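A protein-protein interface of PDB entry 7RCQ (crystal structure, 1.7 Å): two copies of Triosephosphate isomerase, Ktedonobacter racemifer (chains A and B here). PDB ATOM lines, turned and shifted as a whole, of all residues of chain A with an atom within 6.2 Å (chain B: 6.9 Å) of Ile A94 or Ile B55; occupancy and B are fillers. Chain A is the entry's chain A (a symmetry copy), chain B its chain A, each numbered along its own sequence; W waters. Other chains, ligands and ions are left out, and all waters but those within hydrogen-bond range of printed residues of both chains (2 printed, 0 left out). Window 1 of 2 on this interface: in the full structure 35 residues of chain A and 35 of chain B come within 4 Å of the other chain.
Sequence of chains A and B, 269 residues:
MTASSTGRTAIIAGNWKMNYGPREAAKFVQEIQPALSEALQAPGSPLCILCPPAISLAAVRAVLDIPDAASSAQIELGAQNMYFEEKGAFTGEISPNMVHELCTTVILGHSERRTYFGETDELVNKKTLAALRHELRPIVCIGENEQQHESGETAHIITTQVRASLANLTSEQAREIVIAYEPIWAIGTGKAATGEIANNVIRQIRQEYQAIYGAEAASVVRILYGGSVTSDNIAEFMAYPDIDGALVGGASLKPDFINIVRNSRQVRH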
ATOM      1  N   ALA A  54     -11.386  17.702  24.357  1.00  0.00           N
ATOM      2  CA  ALA A  54     -11.219  16.491  23.550  1.00  0.00           C
ATOM      3  C   ALA A  54      -9.766  16.033  23.513  1.00  0.00           C
ATOM      4  O   ALA A  54      -9.493  14.822  23.452  1.00  0.00           O
ATOM      5  CB  ALA A  54     -11.732  16.720  22.125  1.00  0.00           C
ATOM      6  N   ILE A  55      -8.830  16.984  23.534  1.00  0.00           N
ATOM      7  CA  ILE A  55      -7.406  16.670  23.453  1.00  0.00           C
ATOM      8  C   ILE A  55      -6.936  15.935  24.700  1.00  0.00           C
ATOM      9  O   ILE A  55      -5.909  15.242  24.665  1.00  0.00           O
ATOM     10  CB  ILE A  55      -6.623  17.979  23.225  1.00  0.00           C
ATOM     11  CG1 ILE A  55      -5.153  17.714  22.908  1.00  0.00           C
ATOM     12  CG2 ILE A  55      -6.766  18.941  24.435  1.00  0.00           C
ATOM     13  CD1 ILE A  55      -4.445  18.950  22.353  1.00  0.00           C
ATOM     14  N   LEU A  57      -8.942  13.703  26.499  1.00  0.00           N
ATOM     15  CA  LEU A  57      -9.725  12.498  26.775  1.00  0.00           C
ATOM     16  C   LEU A  57      -8.823  11.286  26.989  1.00  0.00           C
ATOM     17  O   LEU A  57      -9.013  10.518  27.934  1.00  0.00           O
ATOM     18  CB  LEU A  57     -10.723  12.250  25.634  1.00  0.00           C
ATOM     19  CG  LEU A  57     -11.910  13.228  25.605  1.00  0.00           C
ATOM     20  CD1 LEU A  57     -12.678  13.136  24.288  1.00  0.00           C
ATOM     21  CD2 LEU A  57     -12.858  12.980  26.756  1.00  0.00           C
ATOM     22  N   ALA A  58      -7.811  11.108  26.135  1.00  0.00           N
ATOM     23  CA  ALA A  58      -6.968   9.921  26.266  1.00  0.00           C
ATOM     24  C   ALA A  58      -6.245   9.902  27.607  1.00  0.00           C
ATOM     25  O   ALA A  58      -6.084   8.839  28.223  1.00  0.00           O
ATOM     26  CB  ALA A  58      -5.958   9.862  25.120  1.00  0.00           C
ATOM     27  N   ALA A  79     -17.633  13.822  25.771  1.00  0.00           N
ATOM     28  CA  ALA A  79     -17.027  14.909  25.017  1.00  0.00           C
ATOM     29  C   ALA A  79     -17.908  16.146  25.113  1.00  0.00           C
ATOM     30  O   ALA A  79     -19.095  16.062  25.442  1.00  0.00           O
ATOM     31  CB  ALA A  79     -16.820  14.516  23.549  1.00  0.00           C
ATOM     32  N   ASN A  81     -18.420  18.357  22.570  1.00  0.00           N
ATOM     33  CA  ASN A  81     -18.957  18.675  21.253  1.00  0.00           C
ATOM     34  C   ASN A  81     -18.407  17.648  20.276  1.00  0.00           C
ATOM     35  O   ASN A  81     -17.357  17.050  20.523  1.00  0.00           O
ATOM     36  CB  ASN A  81     -18.559  20.088  20.815  1.00  0.00           C
ATOM     37  CG  ASN A  81     -19.117  20.450  19.476  1.00  0.00           C
ATOM     38  OD1 ASN A  81     -20.303  20.224  19.213  1.00  0.00           O
ATOM     39  ND2 ASN A  81     -18.269  20.997  18.600  1.00  0.00           N
ATOM     40  N   MET A  82     -19.143  17.432  19.183  1.00  0.00           N
ATOM     41  CA  MET A  82     -18.637  16.717  18.023  1.00  0.00           C
ATOM     42  C   MET A  82     -19.409  17.201  16.805  1.00  0.00           C
ATOM     43  O   MET A  82     -20.394  17.928  16.930  1.00  0.00           O
ATOM     44  CB  MET A  82     -18.808  15.198  18.088  1.00  0.00           C
ATOM     45  CG  MET A  82     -20.251  14.734  17.880  1.00  0.00           C
ATOM     46  SD  MET A  82     -20.590  13.130  18.591  1.00  0.00           S
ATOM     47  CE  MET A  82     -22.323  13.016  18.208  1.00  0.00           C
ATOM     48  N   TYR A  83     -18.979  16.758  15.624  1.00  0.00           N
ATOM     49  CA  TYR A  83     -19.718  17.009  14.390  1.00  0.00           C
ATOM     50  C   TYR A  83     -20.620  15.812  14.069  1.00  0.00           C
ATOM     51  O   TYR A  83     -20.516  14.752  14.688  1.00  0.00           O
ATOM     52  CB  TYR A  83     -18.746  17.295  13.246  1.00  0.00           C
ATOM     53  CG  TYR A  83     -19.370  18.003  12.065  1.00  0.00           C
ATOM     54  CD1 TYR A  83     -20.071  19.185  12.229  1.00  0.00           C
ATOM     55  CD2 TYR A  83     -19.244  17.490  10.783  1.00  0.00           C
ATOM     56  CE1 TYR A  83     -20.644  19.841  11.135  1.00  0.00           C
ATOM     57  CE2 TYR A  83     -19.804  18.137   9.698  1.00  0.00           C
ATOM     58  CZ  TYR A  83     -20.504  19.305   9.876  1.00  0.00           C
ATOM     59  OH  TYR A  83     -21.060  19.942   8.778  1.00  0.00           O
ATOM     60  N   PHE A  84     -21.495  15.965  13.063  1.00  0.00           N
ATOM     61  CA  PHE A  84     -22.526  14.943  12.857  1.00  0.00           C
ATOM     62  C   PHE A  84     -22.251  13.983  11.700  1.00  0.00           C
ATOM     63  O   PHE A  84     -22.903  12.934  11.632  1.00  0.00           O
ATOM     64  CB  PHE A  84     -23.909  15.589  12.642  1.00  0.00           C
ATOM     65  CG  PHE A  84     -23.977  16.492  11.441  1.00  0.00           C
ATOM     66  CD1 PHE A  84     -24.238  15.969  10.178  1.00  0.00           C
ATOM     67  CD2 PHE A  84     -23.788  17.850  11.572  1.00  0.00           C
ATOM     68  CE1 PHE A  84     -24.303  16.796   9.087  1.00  0.00           C
ATOM     69  CE2 PHE A  84     -23.847  18.692  10.464  1.00  0.00           C
ATOM     70  CZ  PHE A  84     -24.103  18.156   9.230  1.00  0.00           C
ATOM     71  N   GLU A  85     -21.332  14.306  10.788  1.00  0.00           N
ATOM     72  CA  GLU A  85     -21.014  13.370   9.717  1.00  0.00           C
ATOM     73  C   GLU A  85     -20.120  12.237  10.233  1.00  0.00           C
ATOM     74  O   GLU A  85     -19.466  12.352  11.270  1.00  0.00           O
ATOM     75  CB  GLU A  85     -20.341  14.097   8.542  1.00  0.00           C
ATOM     76  CG  GLU A  85     -21.144  15.281   7.951  1.00  0.00           C
ATOM     77  CD  GLU A  85     -22.209  14.865   6.942  1.00  0.00           C
ATOM     78  OE1 GLU A  85     -22.472  13.656   6.798  1.00  0.00           O
ATOM     79  OE2 GLU A  85     -22.798  15.756   6.292  1.00  0.00           O
ATOM     80  N   PHE A  90     -13.875  18.080   7.103  1.00  0.00           N
ATOM     81  CA  PHE A  90     -14.341  19.061   8.086  1.00  0.00           C
ATOM     82  C   PHE A  90     -13.176  19.343   9.032  1.00  0.00           C
ATOM     83  O   PHE A  90     -13.144  18.840  10.155  1.00  0.00           O
ATOM     84  CB  PHE A  90     -15.586  18.547   8.811  1.00  0.00           C
ATOM     85  CG  PHE A  90     -16.647  18.061   7.869  1.00  0.00           C
ATOM     86  CD1 PHE A  90     -17.443  18.968   7.197  1.00  0.00           C
ATOM     87  CD2 PHE A  90     -16.805  16.705   7.621  1.00  0.00           C
ATOM     88  CE1 PHE A  90     -18.411  18.532   6.300  1.00  0.00           C
ATOM     89  CE2 PHE A  90     -17.779  16.258   6.728  1.00  0.00           C
ATOM     90  CZ  PHE A  90     -18.575  17.176   6.066  1.00  0.00           C
ATOM     91  N   GLY A  92     -10.779  20.342  11.748  1.00  0.00           N
ATOM     92  CA  GLY A  92     -10.979  20.787  13.111  1.00  0.00           C
ATOM     93  C   GLY A  92     -12.079  20.079  13.871  1.00  0.00           C
ATOM     94  O   GLY A  92     -12.229  20.320  15.084  1.00  0.00           O
ATOM     95  N   GLU A  93     -12.844  19.214  13.210  1.00  0.00           N
ATOM     96  CA  GLU A  93     -13.977  18.545  13.838  1.00  0.00           C
ATOM     97  C   GLU A  93     -13.621  17.108  14.192  1.00  0.00           C
ATOM     98  O   GLU A  93     -12.702  16.509  13.624  1.00  0.00           O
ATOM     99  CB  GLU A  93     -15.203  18.558  12.906  1.00  0.00           C
ATOM    100  CG  GLU A  93     -15.700  19.955  12.579  1.00  0.00           C
ATOM    101  CD  GLU A  93     -16.206  20.663  13.808  1.00  0.00           C
ATOM    102  OE1 GLU A  93     -17.088  20.106  14.492  1.00  0.00           O
ATOM    103  OE2 GLU A  93     -15.700  21.756  14.113  1.00  0.00           O
ATOM    104  N   ILE A  94     -14.365  16.557  15.152  1.00  0.00           N
ATOM    105  CA  ILE A  94     -14.252  15.147  15.509  1.00  0.00           C
ATOM    106  C   ILE A  94     -15.606  14.473  15.292  1.00  0.00           C
ATOM    107  O   ILE A  94     -16.668  15.089  15.440  1.00  0.00           O
ATOM    108  CB  ILE A  94     -13.731  14.934  16.958  1.00  0.00           C
ATOM    109  CG1 ILE A  94     -14.713  15.454  18.010  1.00  0.00           C
ATOM    110  CG2 ILE A  94     -12.381  15.620  17.146  1.00  0.00           C
ATOM    111  CD1 ILE A  94     -14.256  15.139  19.448  1.00  0.00           C
ATOM    112  N   SER A  95     -15.558  13.180  14.922  1.00  0.00           N
ATOM    113  CA  SER A  95     -16.761  12.471  14.497  1.00  0.00           C
ATOM    114  C   SER A  95     -17.334  11.606  15.615  1.00  0.00           C
ATOM    115  O   SER A  95     -16.652  11.311  16.600  1.00  0.00           O
ATOM    116  CB  SER A  95     -16.439  11.591  13.287  1.00  0.00           C
ATOM    117  OG  SER A  95     -15.873  10.372  13.724  1.00  0.00           O
ATOM    118  N   PRO A  96     -18.606  11.187  15.492  1.00  0.00           N
ATOM    119  CA  PRO A  96     -19.211  10.339  16.541  1.00  0.00           C
ATOM    120  C   PRO A  96     -18.451   9.037  16.749  1.00  0.00           C
ATOM    121  O   PRO A  96     -18.306   8.564  17.880  1.00  0.00           O
ATOM    122  CB  PRO A  96     -20.631  10.085  16.019  1.00  0.00           C
ATOM    123  CG  PRO A  96     -20.883  11.113  14.979  1.00  0.00           C
ATOM    124  CD  PRO A  96     -19.551  11.496  14.403  1.00  0.00           C
ATOM    125  N   MET A  98     -15.244   8.614  16.487  1.00  0.00           N
ATOM    126  CA  MET A  98     -14.050   8.936  17.270  1.00  0.00           C
ATOM    127  C   MET A  98     -14.403   9.070  18.740  1.00  0.00           C
ATOM    128  O   MET A  98     -13.723   8.515  19.611  1.00  0.00           O
ATOM    129  CB  MET A  98     -13.480  10.260  16.768  1.00  0.00           C
ATOM    130  CG  MET A  98     -13.213  10.273  15.289  1.00  0.00           C
ATOM    131  SD  MET A  98     -12.281  11.734  14.826  1.00  0.00           S
ATOM    132  CE  MET A  98     -12.116  11.483  13.049  1.00  0.00           C
ATOM    133  N   VAL A  99     -15.458   9.840  19.022  1.00  0.00           N
ATOM    134  CA  VAL A  99     -15.904  10.064  20.393  1.00  0.00           C
ATOM    135  C   VAL A  99     -16.246   8.743  21.064  1.00  0.00           C
ATOM    136  O   VAL A  99     -15.896   8.510  22.227  1.00  0.00           O
ATOM    137  CB  VAL A  99     -17.105  11.029  20.397  1.00  0.00           C
ATOM    138  CG1 VAL A  99     -17.751  11.106  21.796  1.00  0.00           C
ATOM    139  CG2 VAL A  99     -16.658  12.421  19.912  1.00  0.00           C
ATOM    140  N   HIS A 100     -16.930   7.854  20.344  1.00  0.00           N
ATOM    141  CA  HIS A 100     -17.324   6.583  20.939  1.00  0.00           C
ATOM    142  C   HIS A 100     -16.129   5.728  21.364  1.00  0.00           C
ATOM    143  O   HIS A 100     -16.283   4.859  22.231  1.00  0.00           O
ATOM    144  CB  HIS A 100     -18.205   5.803  19.961  1.00  0.00           C
ATOM    145  CG  HIS A 100     -18.792   4.555  20.546  1.00  0.00           C
ATOM    146  ND1 HIS A 100     -18.260   3.304  20.319  1.00  0.00           N
ATOM    147  CD2 HIS A 100     -19.863   4.369  21.353  1.00  0.00           C
ATOM    148  CE1 HIS A 100     -18.979   2.399  20.962  1.00  0.00           C
ATOM    149  NE2 HIS A 100     -19.961   3.019  21.594  1.00  0.00           N
ATOM    150  N   LEU A 102     -13.672   6.592  23.103  1.00  0.00           N
ATOM    151  CA  LEU A 102     -13.222   6.998  24.422  1.00  0.00           C
ATOM    152  C   LEU A 102     -14.341   7.383  25.379  1.00  0.00           C
ATOM    153  O   LEU A 102     -14.071   7.532  26.580  1.00  0.00           O
ATOM    154  CB  LEU A 102     -12.258   8.190  24.307  1.00  0.00           C
ATOM    155  CG  LEU A 102     -10.992   7.989  23.463  1.00  0.00           C
ATOM    156  CD1 LEU A 102     -10.113   9.201  23.607  1.00  0.00           C
ATOM    157  CD2 LEU A 102     -10.231   6.745  23.844  1.00  0.00           C
ATOM    158  N   CYS A 103     -15.574   7.551  24.895  1.00  0.00           N
ATOM    159  CA  CYS A 103     -16.631   8.221  25.642  1.00  0.00           C
ATOM    160  C   CYS A 103     -17.945   7.478  25.492  1.00  0.00           C
ATOM    161  O   CYS A 103     -18.201   6.853  24.466  1.00  0.00           O
ATOM    162  CB  CYS A 103     -16.886   9.636  25.126  1.00  0.00           C
ATOM    163  SG  CYS A 103     -15.444  10.702  25.119  1.00  0.00           S
ATOM    164  N   MET B  18     -11.348  15.324   9.274  1.00  0.00           N
ATOM    165  CA  MET B  18     -12.050  14.548  10.301  1.00  0.00           C
ATOM    166  C   MET B  18     -12.066  13.082   9.864  1.00  0.00           C
ATOM    167  O   MET B  18     -13.048  12.491   9.413  1.00  0.00           O
ATOM    168  CB  MET B  18     -13.414  15.177  10.635  1.00  0.00           C
ATOM    169  CG  MET B  18     -14.360  14.323  11.487  1.00  0.00           C
ATOM    170  SD  MET B  18     -15.973  15.052  11.740  1.00  0.00           S
ATOM    171  CE  MET B  18     -16.945  14.073  10.592  1.00  0.00           C
ATOM    172  N   TYR B  20      -9.791   9.347  11.071  1.00  0.00           N
ATOM    173  CA  TYR B  20      -8.950   8.493  11.905  1.00  0.00           C
ATOM    174  C   TYR B  20      -9.073   8.855  13.379  1.00  0.00           C
ATOM    175  O   TYR B  20      -8.386   9.764  13.853  1.00  0.00           O
ATOM    176  CB  TYR B  20      -7.474   8.518  11.476  1.00  0.00           C
ATOM    177  CG  TYR B  20      -7.210   7.990  10.070  1.00  0.00           C
ATOM    178  CD1 TYR B  20      -8.176   7.279   9.370  1.00  0.00           C
ATOM    179  CD2 TYR B  20      -5.975   8.189   9.462  1.00  0.00           C
ATOM    180  CE1 TYR B  20      -7.922   6.805   8.078  1.00  0.00           C
ATOM    181  CE2 TYR B  20      -5.698   7.702   8.174  1.00  0.00           C
ATOM    182  CZ  TYR B  20      -6.678   7.014   7.491  1.00  0.00           C
ATOM    183  OH  TYR B  20      -6.420   6.534   6.218  1.00  0.00           O
ATOM    184  N   GLY B  21      -9.945   8.126  14.098  1.00  0.00           N
ATOM    185  CA  GLY B  21     -10.021   8.211  15.530  1.00  0.00           C
ATOM    186  C   GLY B  21      -8.784   7.627  16.187  1.00  0.00           C
ATOM    187  O   GLY B  21      -7.831   7.223  15.513  1.00  0.00           O
ATOM    188  N   PRO B  22      -8.773   7.610  17.526  1.00  0.00           N
ATOM    189  CA  PRO B  22      -7.542   7.221  18.241  1.00  0.00           C
ATOM    190  C   PRO B  22      -6.931   5.903  17.773  1.00  0.00           C
ATOM    191  O   PRO B  22      -5.722   5.846  17.490  1.00  0.00           O
ATOM    192  CB  PRO B  22      -8.014   7.163  19.707  1.00  0.00           C
ATOM    193  CG  PRO B  22      -9.069   8.225  19.774  1.00  0.00           C
ATOM    194  CD  PRO B  22      -9.793   8.162  18.441  1.00  0.00           C
ATOM    195  N   PRO B  52      -3.511  15.170  12.936  1.00  0.00           N
ATOM    196  CA  PRO B  52      -4.683  14.320  13.155  1.00  0.00           C
ATOM    197  C   PRO B  52      -5.781  15.070  13.883  1.00  0.00           C
ATOM    198  O   PRO B  52      -5.561  16.186  14.384  1.00  0.00           O
ATOM    199  CB  PRO B  52      -4.132  13.185  14.030  1.00  0.00           C
ATOM    200  CG  PRO B  52      -2.985  13.759  14.727  1.00  0.00           C
ATOM    201  CD  PRO B  52      -2.429  14.894  13.899  1.00  0.00           C
ATOM    202  N   PRO B  53      -6.975  14.476  13.987  1.00  0.00           N
ATOM    203  CA  PRO B  53      -8.015  15.065  14.838  1.00  0.00           C
ATOM    204  C   PRO B  53      -7.524  15.215  16.271  1.00  0.00           C
ATOM    205  O   PRO B  53      -6.703  14.432  16.747  1.00  0.00           O
ATOM    206  CB  PRO B  53      -9.160  14.047  14.756  1.00  0.00           C
ATOM    207  CG  PRO B  53      -8.960  13.350  13.459  1.00  0.00           C
ATOM    208  CD  PRO B  53      -7.447  13.277  13.274  1.00  0.00           C
ATOM    209  N   ALA B  54      -8.072  16.206  16.984  1.00  0.00           N
ATOM    210  CA  ALA B  54      -7.511  16.516  18.301  1.00  0.00           C
ATOM    211  C   ALA B  54      -7.644  15.341  19.262  1.00  0.00           C
ATOM    212  O   ALA B  54      -6.774  15.135  20.124  1.00  0.00           O
ATOM    213  CB  ALA B  54      -8.184  17.757  18.894  1.00  0.00           C
ATOM    214  N   ILE B  55      -8.731  14.576  19.135  1.00  0.00           N
ATOM    215  CA  ILE B  55      -8.993  13.452  20.030  1.00  0.00           C
ATOM    216  C   ILE B  55      -7.973  12.341  19.827  1.00  0.00           C
ATOM    217  O   ILE B  55      -7.770  11.510  20.724  1.00  0.00           O
ATOM    218  CB  ILE B  55     -10.437  12.960  19.796  1.00  0.00           C
ATOM    219  CG1 ILE B  55     -10.864  11.933  20.843  1.00  0.00           C
ATOM    220  CG2 ILE B  55     -10.615  12.395  18.360  1.00  0.00           C
ATOM    221  CD1 ILE B  55     -12.373  11.690  20.836  1.00  0.00           C
ATOM    222  N   SER B  56      -7.296  12.336  18.671  1.00  0.00           N
ATOM    223  CA  SER B  56      -6.354  11.299  18.273  1.00  0.00           C
ATOM    224  C   SER B  56      -4.896  11.702  18.470  1.00  0.00           C
ATOM    225  O   SER B  56      -4.001  10.897  18.192  1.00  0.00           O
ATOM    226  CB  SER B  56      -6.589  10.925  16.801  1.00  0.00           C
ATOM    227  OG  SER B  56      -7.942  10.550  16.577  1.00  0.00           O
ATOM    228  N   LEU B  57      -4.633  12.919  18.963  1.00  0.00           N
ATOM    229  CA  LEU B  57      -3.253  13.385  19.106  1.00  0.00           C
ATOM    230  C   LEU B  57      -2.467  12.506  20.074  1.00  0.00           C
ATOM    231  O   LEU B  57      -1.336  12.109  19.788  1.00  0.00           O
ATOM    232  CB  LEU B  57      -3.240  14.854  19.556  1.00  0.00           C
ATOM    233  CG  LEU B  57      -3.652  15.857  18.464  1.00  0.00           C
ATOM    234  CD1 LEU B  57      -3.926  17.239  19.051  1.00  0.00           C
ATOM    235  CD2 LEU B  57      -2.595  15.969  17.390  1.00  0.00           C
ATOM    236  N   ALA B  58      -3.059  12.165  21.222  1.00  0.00           N
ATOM    237  CA  ALA B  58      -2.312  11.383  22.205  1.00  0.00           C
ATOM    238  C   ALA B  58      -1.920  10.021  21.645  1.00  0.00           C
ATOM    239  O   ALA B  58      -0.819   9.522  21.914  1.00  0.00           O
ATOM    240  CB  ALA B  58      -3.137  11.213  23.481  1.00  0.00           C
ATOM    241  N   ALA B  59      -2.819   9.397  20.885  1.00  0.00           N
ATOM    242  CA  ALA B  59      -2.523   8.078  20.333  1.00  0.00           C
ATOM    243  C   ALA B  59      -1.366   8.150  19.343  1.00  0.00           C
ATOM    244  O   ALA B  59      -0.507   7.261  19.311  1.00  0.00           O
ATOM    245  CB  ALA B  59      -3.772   7.499  19.667  1.00  0.00           C
HETATM  246  O   HOH W   1      -5.332  13.655  22.325  1.00  0.00           O
HETATM  247  O   HOH W   2      -7.750  12.357  23.482  1.00  0.00           O
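The side-chain sulfur (SD) of Met B18 is in hydrogen-bond range of the backbone NH (N) of Ser A95 (3.7 Å).
The backbone carbonyl oxygen (O) of Ile A94 lies close to the side-chain sulfur (SD) of Met B18 (3.8 Å).
O of Tyr B20 lies within hydrogen-bond range of OG of Ser B56.
O of Gly B21 sits close to OG of Ser B56, at 3.5 Å.
O of Ile A94 lies within hydrogen-bond range of N of Tyr A83.
OG of Ser A95 lies close to N of Met A98 (3.3 Å).
SG of Cys A103 lies close to O of Val A99 (3.7 Å).
Among the printed residues, merely in contact across the chains: Ala A54 with Ile B55, Ile A55 with Ala B54, Ile A55 with Leu B57, Leu A57 with Ile B55, Ala A58 with Ala B58, Tyr A83 with Met B18, Glu A85 with Met B18, Phe A90 with Met B18, Glu A93 with Met B18, Ile A94 with Ile B55, Met A98 with Met B18, Met A98 with Tyr B20, Met A98 with Gly B21, Met A98 with Pro B53, Met A98 with Ile B55, Val A99 with Ile B55 and Leu A102 with Ile B55.
Of the printed residues of chain B, Ile A55 touches Ala B54 and Leu B57.
Asn A81 touches none of the printed residues of chain B.
Printed residues of chain B within 4 Å of Tyr A83: Met B18.
Ile A94 touches two residues of chain B.
Pro B22 touches none of the printed residues of chain A.
Of the printed residues of chain A, Ala B54 touches Ile A55.
Ile B55 touches six residues of chain A.
Of the printed residues of chain A, Leu B57 touches Ile A55.
Printed residues of chain A within 4 Å of Ala B58: Ala A58 (3.5 Å).
The nearest residue of chain B that does not touch Ile A94 is Pro B53 (4.3 Å).
The nearest residue of chain A that does not touch Ile B55 is Ile A55 (5.0 Å).
Of the 12 printed residues of chain B, 8 touch a printed residue of chain A.
Hydrophobic or aromatic side chains of chain B within 4 Å of the printed part of chain A: Met B18, Pro B53, Ile B55, Leu B57 and Ala B58.
Along chain B the printed residues that touch a printed residue of chain A span positions 18 to 58.
Among the printed residues, no Asp or Glu carboxylate lies within 4 Å of a Lys or Arg side-chain nitrogen of the other chain.
Ala A54 touches Ile B55, and with the chains exchanged Ile A55 touches Ala B54.
Ile A55 touches Leu B57, and with the chains exchanged Leu A57 touches Ile B55.
Ala A58 touches its own counterpart, Ala B58.
Water W2 lies within hydrogen-bond range of O of Ile B55, N of Ala A58 and O of Ala A54.
Water W1 lies within hydrogen-bond range of the backbone carbonyl oxygen of Ile A55 (2.9 Å), the backbone NH of Ala B58 (2.9 Å) and the backbone carbonyl oxygen of Ala B54 (3.0 Å).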
